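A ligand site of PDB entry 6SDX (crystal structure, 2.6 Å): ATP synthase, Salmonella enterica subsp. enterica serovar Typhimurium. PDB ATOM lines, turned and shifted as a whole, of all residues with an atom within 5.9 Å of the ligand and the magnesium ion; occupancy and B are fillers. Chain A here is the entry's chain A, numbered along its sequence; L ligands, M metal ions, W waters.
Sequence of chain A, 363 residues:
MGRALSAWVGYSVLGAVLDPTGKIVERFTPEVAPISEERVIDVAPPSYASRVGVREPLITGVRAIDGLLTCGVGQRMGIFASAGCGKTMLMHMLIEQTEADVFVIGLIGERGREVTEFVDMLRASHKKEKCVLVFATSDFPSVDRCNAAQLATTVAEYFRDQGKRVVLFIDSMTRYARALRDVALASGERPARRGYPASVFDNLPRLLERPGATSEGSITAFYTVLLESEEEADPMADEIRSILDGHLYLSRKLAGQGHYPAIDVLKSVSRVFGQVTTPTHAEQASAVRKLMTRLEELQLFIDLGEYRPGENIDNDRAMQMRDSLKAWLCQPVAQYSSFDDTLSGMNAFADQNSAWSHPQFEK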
ATOM      1  N   ALA A  81      30.989   4.132  16.519  1.00  0.00           N
ATOM      2  CA  ALA A  81      30.063   3.224  15.852  1.00  0.00           C
ATOM      3  C   ALA A  81      29.449   3.930  14.659  1.00  0.00           C
ATOM      4  O   ALA A  81      29.311   5.160  14.647  1.00  0.00           O
ATOM      5  CB  ALA A  81      28.966   2.739  16.808  1.00  0.00           C
ATOM      6  N   SER A  82      29.084   3.138  13.653  1.00  0.00           N
ATOM      7  CA  SER A  82      28.235   3.643  12.584  1.00  0.00           C
ATOM      8  C   SER A  82      26.811   3.760  13.112  1.00  0.00           C
ATOM      9  O   SER A  82      26.590   3.757  14.323  1.00  0.00           O
ATOM     10  CB  SER A  82      28.298   2.716  11.358  1.00  0.00           C
ATOM     11  OG  SER A  82      27.706   1.461  11.625  1.00  0.00           O
ATOM     12  N   ALA A  83      25.833   3.866  12.213  1.00  0.00           N
ATOM     13  CA  ALA A  83      24.464   4.079  12.641  1.00  0.00           C
ATOM     14  C   ALA A  83      23.822   2.773  13.101  1.00  0.00           C
ATOM     15  O   ALA A  83      24.087   1.696  12.566  1.00  0.00           O
ATOM     16  CB  ALA A  83      23.639   4.700  11.517  1.00  0.00           C
ATOM     17  N   GLY A  84      22.979   2.892  14.125  1.00  0.00           N
ATOM     18  CA  GLY A  84      22.171   1.769  14.594  1.00  0.00           C
ATOM     19  C   GLY A  84      22.896   0.752  15.428  1.00  0.00           C
ATOM     20  O   GLY A  84      22.348  -0.336  15.657  1.00  0.00           O
ATOM     21  N   CYS A  85      24.107   1.040  15.893  1.00  0.00           N
ATOM     22  CA  CYS A  85      24.903   0.082  16.645  1.00  0.00           C
ATOM     23  C   CYS A  85      24.732   0.205  18.155  1.00  0.00           C
ATOM     24  O   CYS A  85      25.264  -0.628  18.895  1.00  0.00           O
ATOM     25  CB  CYS A  85      26.388   0.223  16.281  1.00  0.00           C
ATOM     26  SG  CYS A  85      26.748   0.013  14.521  1.00  0.00           S
ATOM     27  N   GLY A  86      24.022   1.223  18.639  1.00  0.00           N
ATOM     28  CA  GLY A  86      23.689   1.334  20.032  1.00  0.00           C
ATOM     29  C   GLY A  86      24.505   2.302  20.861  1.00  0.00           C
ATOM     30  O   GLY A  86      24.741   2.020  22.043  1.00  0.00           O
ATOM     31  N   LYS A  87      24.936   3.425  20.285  1.00  0.00           N
ATOM     32  CA  LYS A  87      25.706   4.392  21.056  1.00  0.00           C
ATOM     33  C   LYS A  87      24.866   5.018  22.167  1.00  0.00           C
ATOM     34  O   LYS A  87      25.279   5.071  23.323  1.00  0.00           O
ATOM     35  CB  LYS A  87      26.281   5.467  20.123  1.00  0.00           C
ATOM     36  CG  LYS A  87      27.311   4.948  19.132  1.00  0.00           C
ATOM     37  CD  LYS A  87      27.923   6.078  18.319  1.00  0.00           C
ATOM     38  CE  LYS A  87      27.019   6.533  17.184  1.00  0.00           C
ATOM     39  NZ  LYS A  87      26.967   5.532  16.078  1.00  0.00           N
ATOM     40  N   THR A  88      23.661   5.488  21.810  1.00  0.00           N
ATOM     41  CA  THR A  88      22.773   6.087  22.807  1.00  0.00           C
ATOM     42  C   THR A  88      22.372   5.086  23.880  1.00  0.00           C
ATOM     43  O   THR A  88      22.317   5.422  25.077  1.00  0.00           O
ATOM     44  CB  THR A  88      21.532   6.658  22.107  1.00  0.00           C
ATOM     45  OG1 THR A  88      21.911   7.778  21.287  1.00  0.00           O
ATOM     46  CG2 THR A  88      20.502   7.108  23.120  1.00  0.00           C
ATOM     47  N   MET A  89      22.098   3.848  23.486  1.00  0.00           N
ATOM     48  CA  MET A  89      21.726   2.832  24.470  1.00  0.00           C
ATOM     49  C   MET A  89      22.903   2.499  25.380  1.00  0.00           C
ATOM     50  O   MET A  89      22.724   2.250  26.571  1.00  0.00           O
ATOM     51  CB  MET A  89      21.220   1.577  23.763  1.00  0.00           C
ATOM     52  CG  MET A  89      19.874   1.771  23.073  1.00  0.00           C
ATOM     53  SD  MET A  89      18.577   2.215  24.232  1.00  0.00           S
ATOM     54  CE  MET A  89      18.651   0.824  25.358  1.00  0.00           C
ATOM     55  N   LEU A  90      24.126   2.497  24.835  1.00  0.00           N
ATOM     56  CA  LEU A  90      25.307   2.303  25.672  1.00  0.00           C
ATOM     57  C   LEU A  90      25.461   3.451  26.664  1.00  0.00           C
ATOM     58  O   LEU A  90      25.832   3.222  27.823  1.00  0.00           O
ATOM     59  CB  LEU A  90      26.550   2.172  24.788  1.00  0.00           C
ATOM     60  CG  LEU A  90      27.869   1.844  25.497  1.00  0.00           C
ATOM     61  CD1 LEU A  90      27.673   0.738  26.523  1.00  0.00           C
ATOM     62  CD2 LEU A  90      28.911   1.444  24.478  1.00  0.00           C
ATOM     63  N   MET A  91      25.167   4.675  26.228  1.00  0.00           N
ATOM     64  CA  MET A  91      25.144   5.816  27.143  1.00  0.00           C
ATOM     65  C   MET A  91      24.141   5.590  28.267  1.00  0.00           C
ATOM     66  O   MET A  91      24.441   5.849  29.439  1.00  0.00           O
ATOM     67  CB  MET A  91      24.789   7.090  26.390  1.00  0.00           C
ATOM     68  CG  MET A  91      25.772   7.521  25.318  1.00  0.00           C
ATOM     69  SD  MET A  91      25.126   8.931  24.398  1.00  0.00           S
ATOM     70  CE  MET A  91      24.611  10.000  25.747  1.00  0.00           C
ATOM     71  N   GLU A 110      20.635  16.438  17.461  1.00  0.00           N
ATOM     72  CA  GLU A 110      19.718  15.346  17.163  1.00  0.00           C
ATOM     73  C   GLU A 110      18.315  15.891  16.946  1.00  0.00           C
ATOM     74  O   GLU A 110      18.022  17.063  17.212  1.00  0.00           O
ATOM     75  CB  GLU A 110      19.721  14.313  18.296  1.00  0.00           C
ATOM     76  CG  GLU A 110      20.612  13.108  18.049  1.00  0.00           C
ATOM     77  CD  GLU A 110      19.999  12.102  17.073  1.00  0.00           C
ATOM     78  OE1 GLU A 110      20.646  11.068  16.809  1.00  0.00           O
ATOM     79  OE2 GLU A 110      18.881  12.360  16.574  1.00  0.00           O
ATOM     80  N   GLU A 114      14.235  12.773  19.603  1.00  0.00           N
ATOM     81  CA  GLU A 114      15.276  12.009  20.290  1.00  0.00           C
ATOM     82  C   GLU A 114      15.605  12.637  21.641  1.00  0.00           C
ATOM     83  O   GLU A 114      15.812  11.933  22.638  1.00  0.00           O
ATOM     84  CB  GLU A 114      16.519  11.908  19.419  1.00  0.00           C
ATOM     85  CG  GLU A 114      16.261  11.289  18.057  1.00  0.00           C
ATOM     86  CD  GLU A 114      16.029   9.796  18.115  1.00  0.00           C
ATOM     87  OE1 GLU A 114      16.897   9.095  18.675  1.00  0.00           O
ATOM     88  OE2 GLU A 114      14.977   9.330  17.626  1.00  0.00           O
ATOM     89  N   ASP A 171      27.032  13.479  22.823  1.00  0.00           N
ATOM     90  CA  ASP A 171      26.449  12.792  21.676  1.00  0.00           C
ATOM     91  C   ASP A 171      25.956  13.872  20.719  1.00  0.00           C
ATOM     92  O   ASP A 171      24.903  14.479  20.955  1.00  0.00           O
ATOM     93  CB  ASP A 171      25.306  11.878  22.114  1.00  0.00           C
ATOM     94  CG  ASP A 171      24.880  10.891  21.052  1.00  0.00           C
ATOM     95  OD1 ASP A 171      24.501   9.758  21.407  1.00  0.00           O
ATOM     96  OD2 ASP A 171      24.949  11.239  19.850  1.00  0.00           O
ATOM     97  N   ARG A 175      28.959  15.707  15.367  1.00  0.00           N
ATOM     98  CA  ARG A 175      28.119  16.871  15.107  1.00  0.00           C
ATOM     99  C   ARG A 175      28.727  18.137  15.687  1.00  0.00           C
ATOM    100  O   ARG A 175      28.593  19.218  15.098  1.00  0.00           O
ATOM    101  CB  ARG A 175      26.716  16.632  15.664  1.00  0.00           C
ATOM    102  CG  ARG A 175      25.993  15.473  14.988  1.00  0.00           C
ATOM    103  CD  ARG A 175      24.512  15.492  15.330  1.00  0.00           C
ATOM    104  NE  ARG A 175      23.726  14.532  14.542  1.00  0.00           N
ATOM    105  CZ  ARG A 175      23.269  13.387  15.021  1.00  0.00           C
ATOM    106  NH1 ARG A 175      23.497  13.042  16.289  1.00  0.00           N
ATOM    107  NH2 ARG A 175      22.565  12.576  14.244  1.00  0.00           N
ATOM    108  N   THR A 224      30.666  10.219  21.779  1.00  0.00           N
ATOM    109  CA  THR A 224      30.237   9.349  20.694  1.00  0.00           C
ATOM    110  C   THR A 224      30.713   9.911  19.358  1.00  0.00           C
ATOM    111  O   THR A 224      30.611  11.115  19.116  1.00  0.00           O
ATOM    112  CB  THR A 224      28.717   9.173  20.688  1.00  0.00           C
ATOM    113  OG1 THR A 224      28.115  10.387  20.235  1.00  0.00           O
ATOM    114  CG2 THR A 224      28.222   8.875  22.090  1.00  0.00           C
ATOM    115  N   LEU A 226      30.529   9.143  15.126  1.00  0.00           N
ATOM    116  CA  LEU A 226      29.879   8.402  14.056  1.00  0.00           C
ATOM    117  C   LEU A 226      30.906   7.963  13.021  1.00  0.00           C
ATOM    118  O   LEU A 226      31.747   8.757  12.581  1.00  0.00           O
ATOM    119  CB  LEU A 226      28.796   9.252  13.384  1.00  0.00           C
ATOM    120  CG  LEU A 226      28.023   8.525  12.288  1.00  0.00           C
ATOM    121  CD1 LEU A 226      27.393   7.256  12.836  1.00  0.00           C
ATOM    122  CD2 LEU A 226      26.962   9.424  11.676  1.00  0.00           C
ATOM    123  N   TYR A 260      24.214  -7.194  22.557  1.00  0.00           N
ATOM    124  CA  TYR A 260      24.352  -5.871  23.137  1.00  0.00           C
ATOM    125  C   TYR A 260      24.984  -5.944  24.520  1.00  0.00           C
ATOM    126  O   TYR A 260      24.656  -6.853  25.302  1.00  0.00           O
ATOM    127  CB  TYR A 260      22.981  -5.181  23.245  1.00  0.00           C
ATOM    128  CG  TYR A 260      22.329  -4.904  21.914  1.00  0.00           C
ATOM    129  CD1 TYR A 260      22.958  -4.096  20.964  1.00  0.00           C
ATOM    130  CD2 TYR A 260      21.079  -5.406  21.610  1.00  0.00           C
ATOM    131  CE1 TYR A 260      22.362  -3.824  19.749  1.00  0.00           C
ATOM    132  CE2 TYR A 260      20.470  -5.138  20.400  1.00  0.00           C
ATOM    133  CZ  TYR A 260      21.121  -4.347  19.475  1.00  0.00           C
ATOM    134  OH  TYR A 260      20.525  -4.076  18.259  1.00  0.00           O
ATOM    135  N   PRO A 261      25.909  -5.026  24.864  1.00  0.00           N
ATOM    136  CA  PRO A 261      26.429  -3.948  24.009  1.00  0.00           C
ATOM    137  C   PRO A 261      27.255  -4.474  22.837  1.00  0.00           C
ATOM    138  O   PRO A 261      27.964  -5.464  22.997  1.00  0.00           O
ATOM    139  CB  PRO A 261      27.308  -3.127  24.955  1.00  0.00           C
ATOM    140  CG  PRO A 261      26.817  -3.455  26.315  1.00  0.00           C
ATOM    141  CD  PRO A 261      26.397  -4.894  26.245  1.00  0.00           C
ATOM    142  N   ALA A 262      27.159  -3.823  21.686  1.00  0.00           N
ATOM    143  CA  ALA A 262      27.762  -4.352  20.459  1.00  0.00           C
ATOM    144  C   ALA A 262      29.258  -4.111  20.439  1.00  0.00           C
ATOM    145  O   ALA A 262      29.834  -3.834  19.379  1.00  0.00           O
ATOM    146  CB  ALA A 262      27.109  -3.727  19.225  1.00  0.00           C
ATOM    147  N   GLN A 331      25.077  -8.434  27.627  1.00  0.00           N
ATOM    148  CA  GLN A 331      24.554  -7.979  28.916  1.00  0.00           C
ATOM    149  C   GLN A 331      23.509  -6.887  28.727  1.00  0.00           C
ATOM    150  O   GLN A 331      23.785  -5.871  28.079  1.00  0.00           O
ATOM    151  CB  GLN A 331      25.701  -7.487  29.785  1.00  0.00           C
ATOM    152  CG  GLN A 331      25.284  -6.894  31.118  1.00  0.00           C
ATOM    153  CD  GLN A 331      26.453  -6.289  31.867  1.00  0.00           C
ATOM    154  OE1 GLN A 331      27.607  -6.431  31.462  1.00  0.00           O
ATOM    155  NE2 GLN A 331      26.164  -5.607  32.968  1.00  0.00           N
ATOM    156  N   VAL A 333      20.758  -3.739  29.361  1.00  0.00           N
ATOM    157  CA  VAL A 333      20.942  -2.396  29.911  1.00  0.00           C
ATOM    158  C   VAL A 333      20.635  -2.393  31.410  1.00  0.00           C
ATOM    159  O   VAL A 333      21.384  -1.825  32.218  1.00  0.00           O
ATOM    160  CB  VAL A 333      20.072  -1.378  29.162  1.00  0.00           C
ATOM    161  CG1 VAL A 333      20.098  -0.039  29.875  1.00  0.00           C
ATOM    162  CG2 VAL A 333      20.553  -1.233  27.724  1.00  0.00           C
HETATM  163  P1  LIG L   1      22.117   6.902  16.014  1.00  0.00           P
HETATM  164  S1  LIG L   1      23.624   6.903  14.775  1.00  0.00           S
HETATM  165  O1  LIG L   1      20.833   7.349  15.259  1.00  0.00           O
HETATM  166  O2  LIG L   1      22.408   7.933  17.149  1.00  0.00           O
HETATM  167  P2  LIG L   1      22.902   4.808  17.641  1.00  0.00           P
HETATM  168  O3  LIG L   1      24.204   4.512  16.989  1.00  0.00           O
HETATM  169  O4  LIG L   1      23.050   5.757  18.841  1.00  0.00           O
HETATM  170  O5  LIG L   1      21.898   5.483  16.618  1.00  0.00           O
HETATM  171  P3  LIG L   1      20.987   3.558  19.182  1.00  0.00           P
HETATM  172  O6  LIG L   1      21.420   3.467  20.599  1.00  0.00           O
HETATM  173  O7  LIG L   1      20.265   4.863  18.824  1.00  0.00           O
HETATM  174  O8  LIG L   1      22.254   3.477  18.207  1.00  0.00           O
HETATM  175  O9  LIG L   1      20.067   2.300  18.870  1.00  0.00           O
HETATM  176  C1  LIG L   1      18.632   2.456  18.724  1.00  0.00           C
HETATM  177  C2  LIG L   1      17.939   1.112  18.698  1.00  0.00           C
HETATM  178  O10 LIG L   1      18.906   0.057  18.503  1.00  0.00           O
HETATM  179  C3  LIG L   1      17.191   0.742  19.976  1.00  0.00           C
HETATM  180  O11 LIG L   1      15.850   1.243  19.948  1.00  0.00           O
HETATM  181  C4  LIG L   1      17.224  -0.779  19.946  1.00  0.00           C
HETATM  182  O12 LIG L   1      16.199  -1.331  19.118  1.00  0.00           O
HETATM  183  C5  LIG L   1      18.609  -1.044  19.342  1.00  0.00           C
HETATM  184  N1  LIG L   1      19.681  -1.148  20.341  1.00  0.00           N
HETATM  185  C6  LIG L   1      20.901  -0.545  20.261  1.00  0.00           C
HETATM  186  N2  LIG L   1      21.692  -0.793  21.277  1.00  0.00           N
HETATM  187  C7  LIG L   1      20.932  -1.625  22.086  1.00  0.00           C
HETATM  188  C8  LIG L   1      21.181  -2.244  23.324  1.00  0.00           C
HETATM  189  N3  LIG L   1      22.337  -2.113  23.997  1.00  0.00           N
HETATM  190  N4  LIG L   1      20.205  -3.010  23.864  1.00  0.00           N
HETATM  191  C9  LIG L   1      19.059  -3.138  23.200  1.00  0.00           C
HETATM  192  N5  LIG L   1      18.698  -2.606  22.024  1.00  0.00           N
HETATM  193  C10 LIG L   1      19.684  -1.854  21.522  1.00  0.00           C
HETATM  194 MG    MG M   1      23.250   8.548  19.121  1.00  0.00          MG
HETATM  195  O   HOH W   1      20.609   7.725  19.076  1.00  0.00           O
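Merely in contact with the ligand: Tyr 260 (3.2 Å), Gly 84 (3.5 Å), Glu 110 (3.6 Å), Ala 83 (3.6 Å), Cys 85 (3.6 Å) and Ser 82 (3.7 Å).
Within 4 Å of the ligand: Ser 82, Ala 83, Gly 84, Cys 85, Gly 86, Lys 87, Thr 88, Met 89, Glu 110 and Tyr 260.
The magnesium ion is bound by O2 of the ligand (2.2 Å).
Slightly farther from the magnesium ion lies the side-chain hydroxyl (OG1) of Thr 88 (2.7 Å).
Slightly farther from the magnesium ion lies water W1 (2.8 Å).
Slightly farther from the magnesium ion lies an oxygen (O4) of the ligand (2.8 Å).
An oxygen (O4) of the ligand is in hydrogen-bond range of the backbone NH of Thr 88, 3.0 Å away.
The side-chain hydroxyl (OG1) of Thr 88 is in hydrogen-bond range of an oxygen (O4) of the ligand, at 3.4 Å.
The backbone NH of Gly 86 is in hydrogen-bond range of an oxygen (O8) of the ligand, at 2.9 Å.
O6 of the ligand sits at hydrogen-bond distance from N of Met 89 (3.0 Å).
The backbone NH (N) of Lys 87 sits at hydrogen-bond distance from an oxygen (O4) of the ligand, at 3.3 Å.
NZ of Lys 87 lies within salt-bridge range of O3 of the ligand, 3.1 Å away.
The side-chain carboxylate (OD1) of Asp 171 sits at hydrogen-bond distance from the side-chain hydroxyl (OG1) of Thr 88 (3.3 Å).
The side-chain hydroxyl (OG1) of Thr 224 lies close to the side-chain carboxylate (OD2) of Asp 171, 3.3 Å away.
The backbone carbonyl oxygen (O) of Ser 82 sits at hydrogen-bond distance from the side-chain amino group (NZ) of Lys 87 (2.5 Å).
The side-chain amino group of Lys 87 is in hydrogen-bond range of the backbone carbonyl oxygen of Ala 81 (2.8 Å).
N of Gln 331 is in hydrogen-bond range of O of Tyr 260.
The guanidinium group (NH1) of Arg 175 is in salt-bridge range of the side-chain carboxylate (OE1) of Glu 110 (3.5 Å).
The backbone carbonyl oxygen (O) of Ala 83 is in hydrogen-bond range of the side-chain sulfur (SG) of Cys 85, at 3.7 Å.
The side-chain sulfur of Cys 85 is in hydrogen-bond range of the side-chain hydroxyl of Ser 82 (3.4 Å).
Residues that only touch the magnesium ion: Asp 171.
Two residues have an atom within 4 Å of the magnesium ion: Thr 88 and Asp 171.
The nearest printed residue that does not touch the magnesium ion is Glu 110 (4.3 Å).
Water W1 bridges the side-chain hydroxyl (OG1) of Thr 88 and an oxygen (O7) of the ligand.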
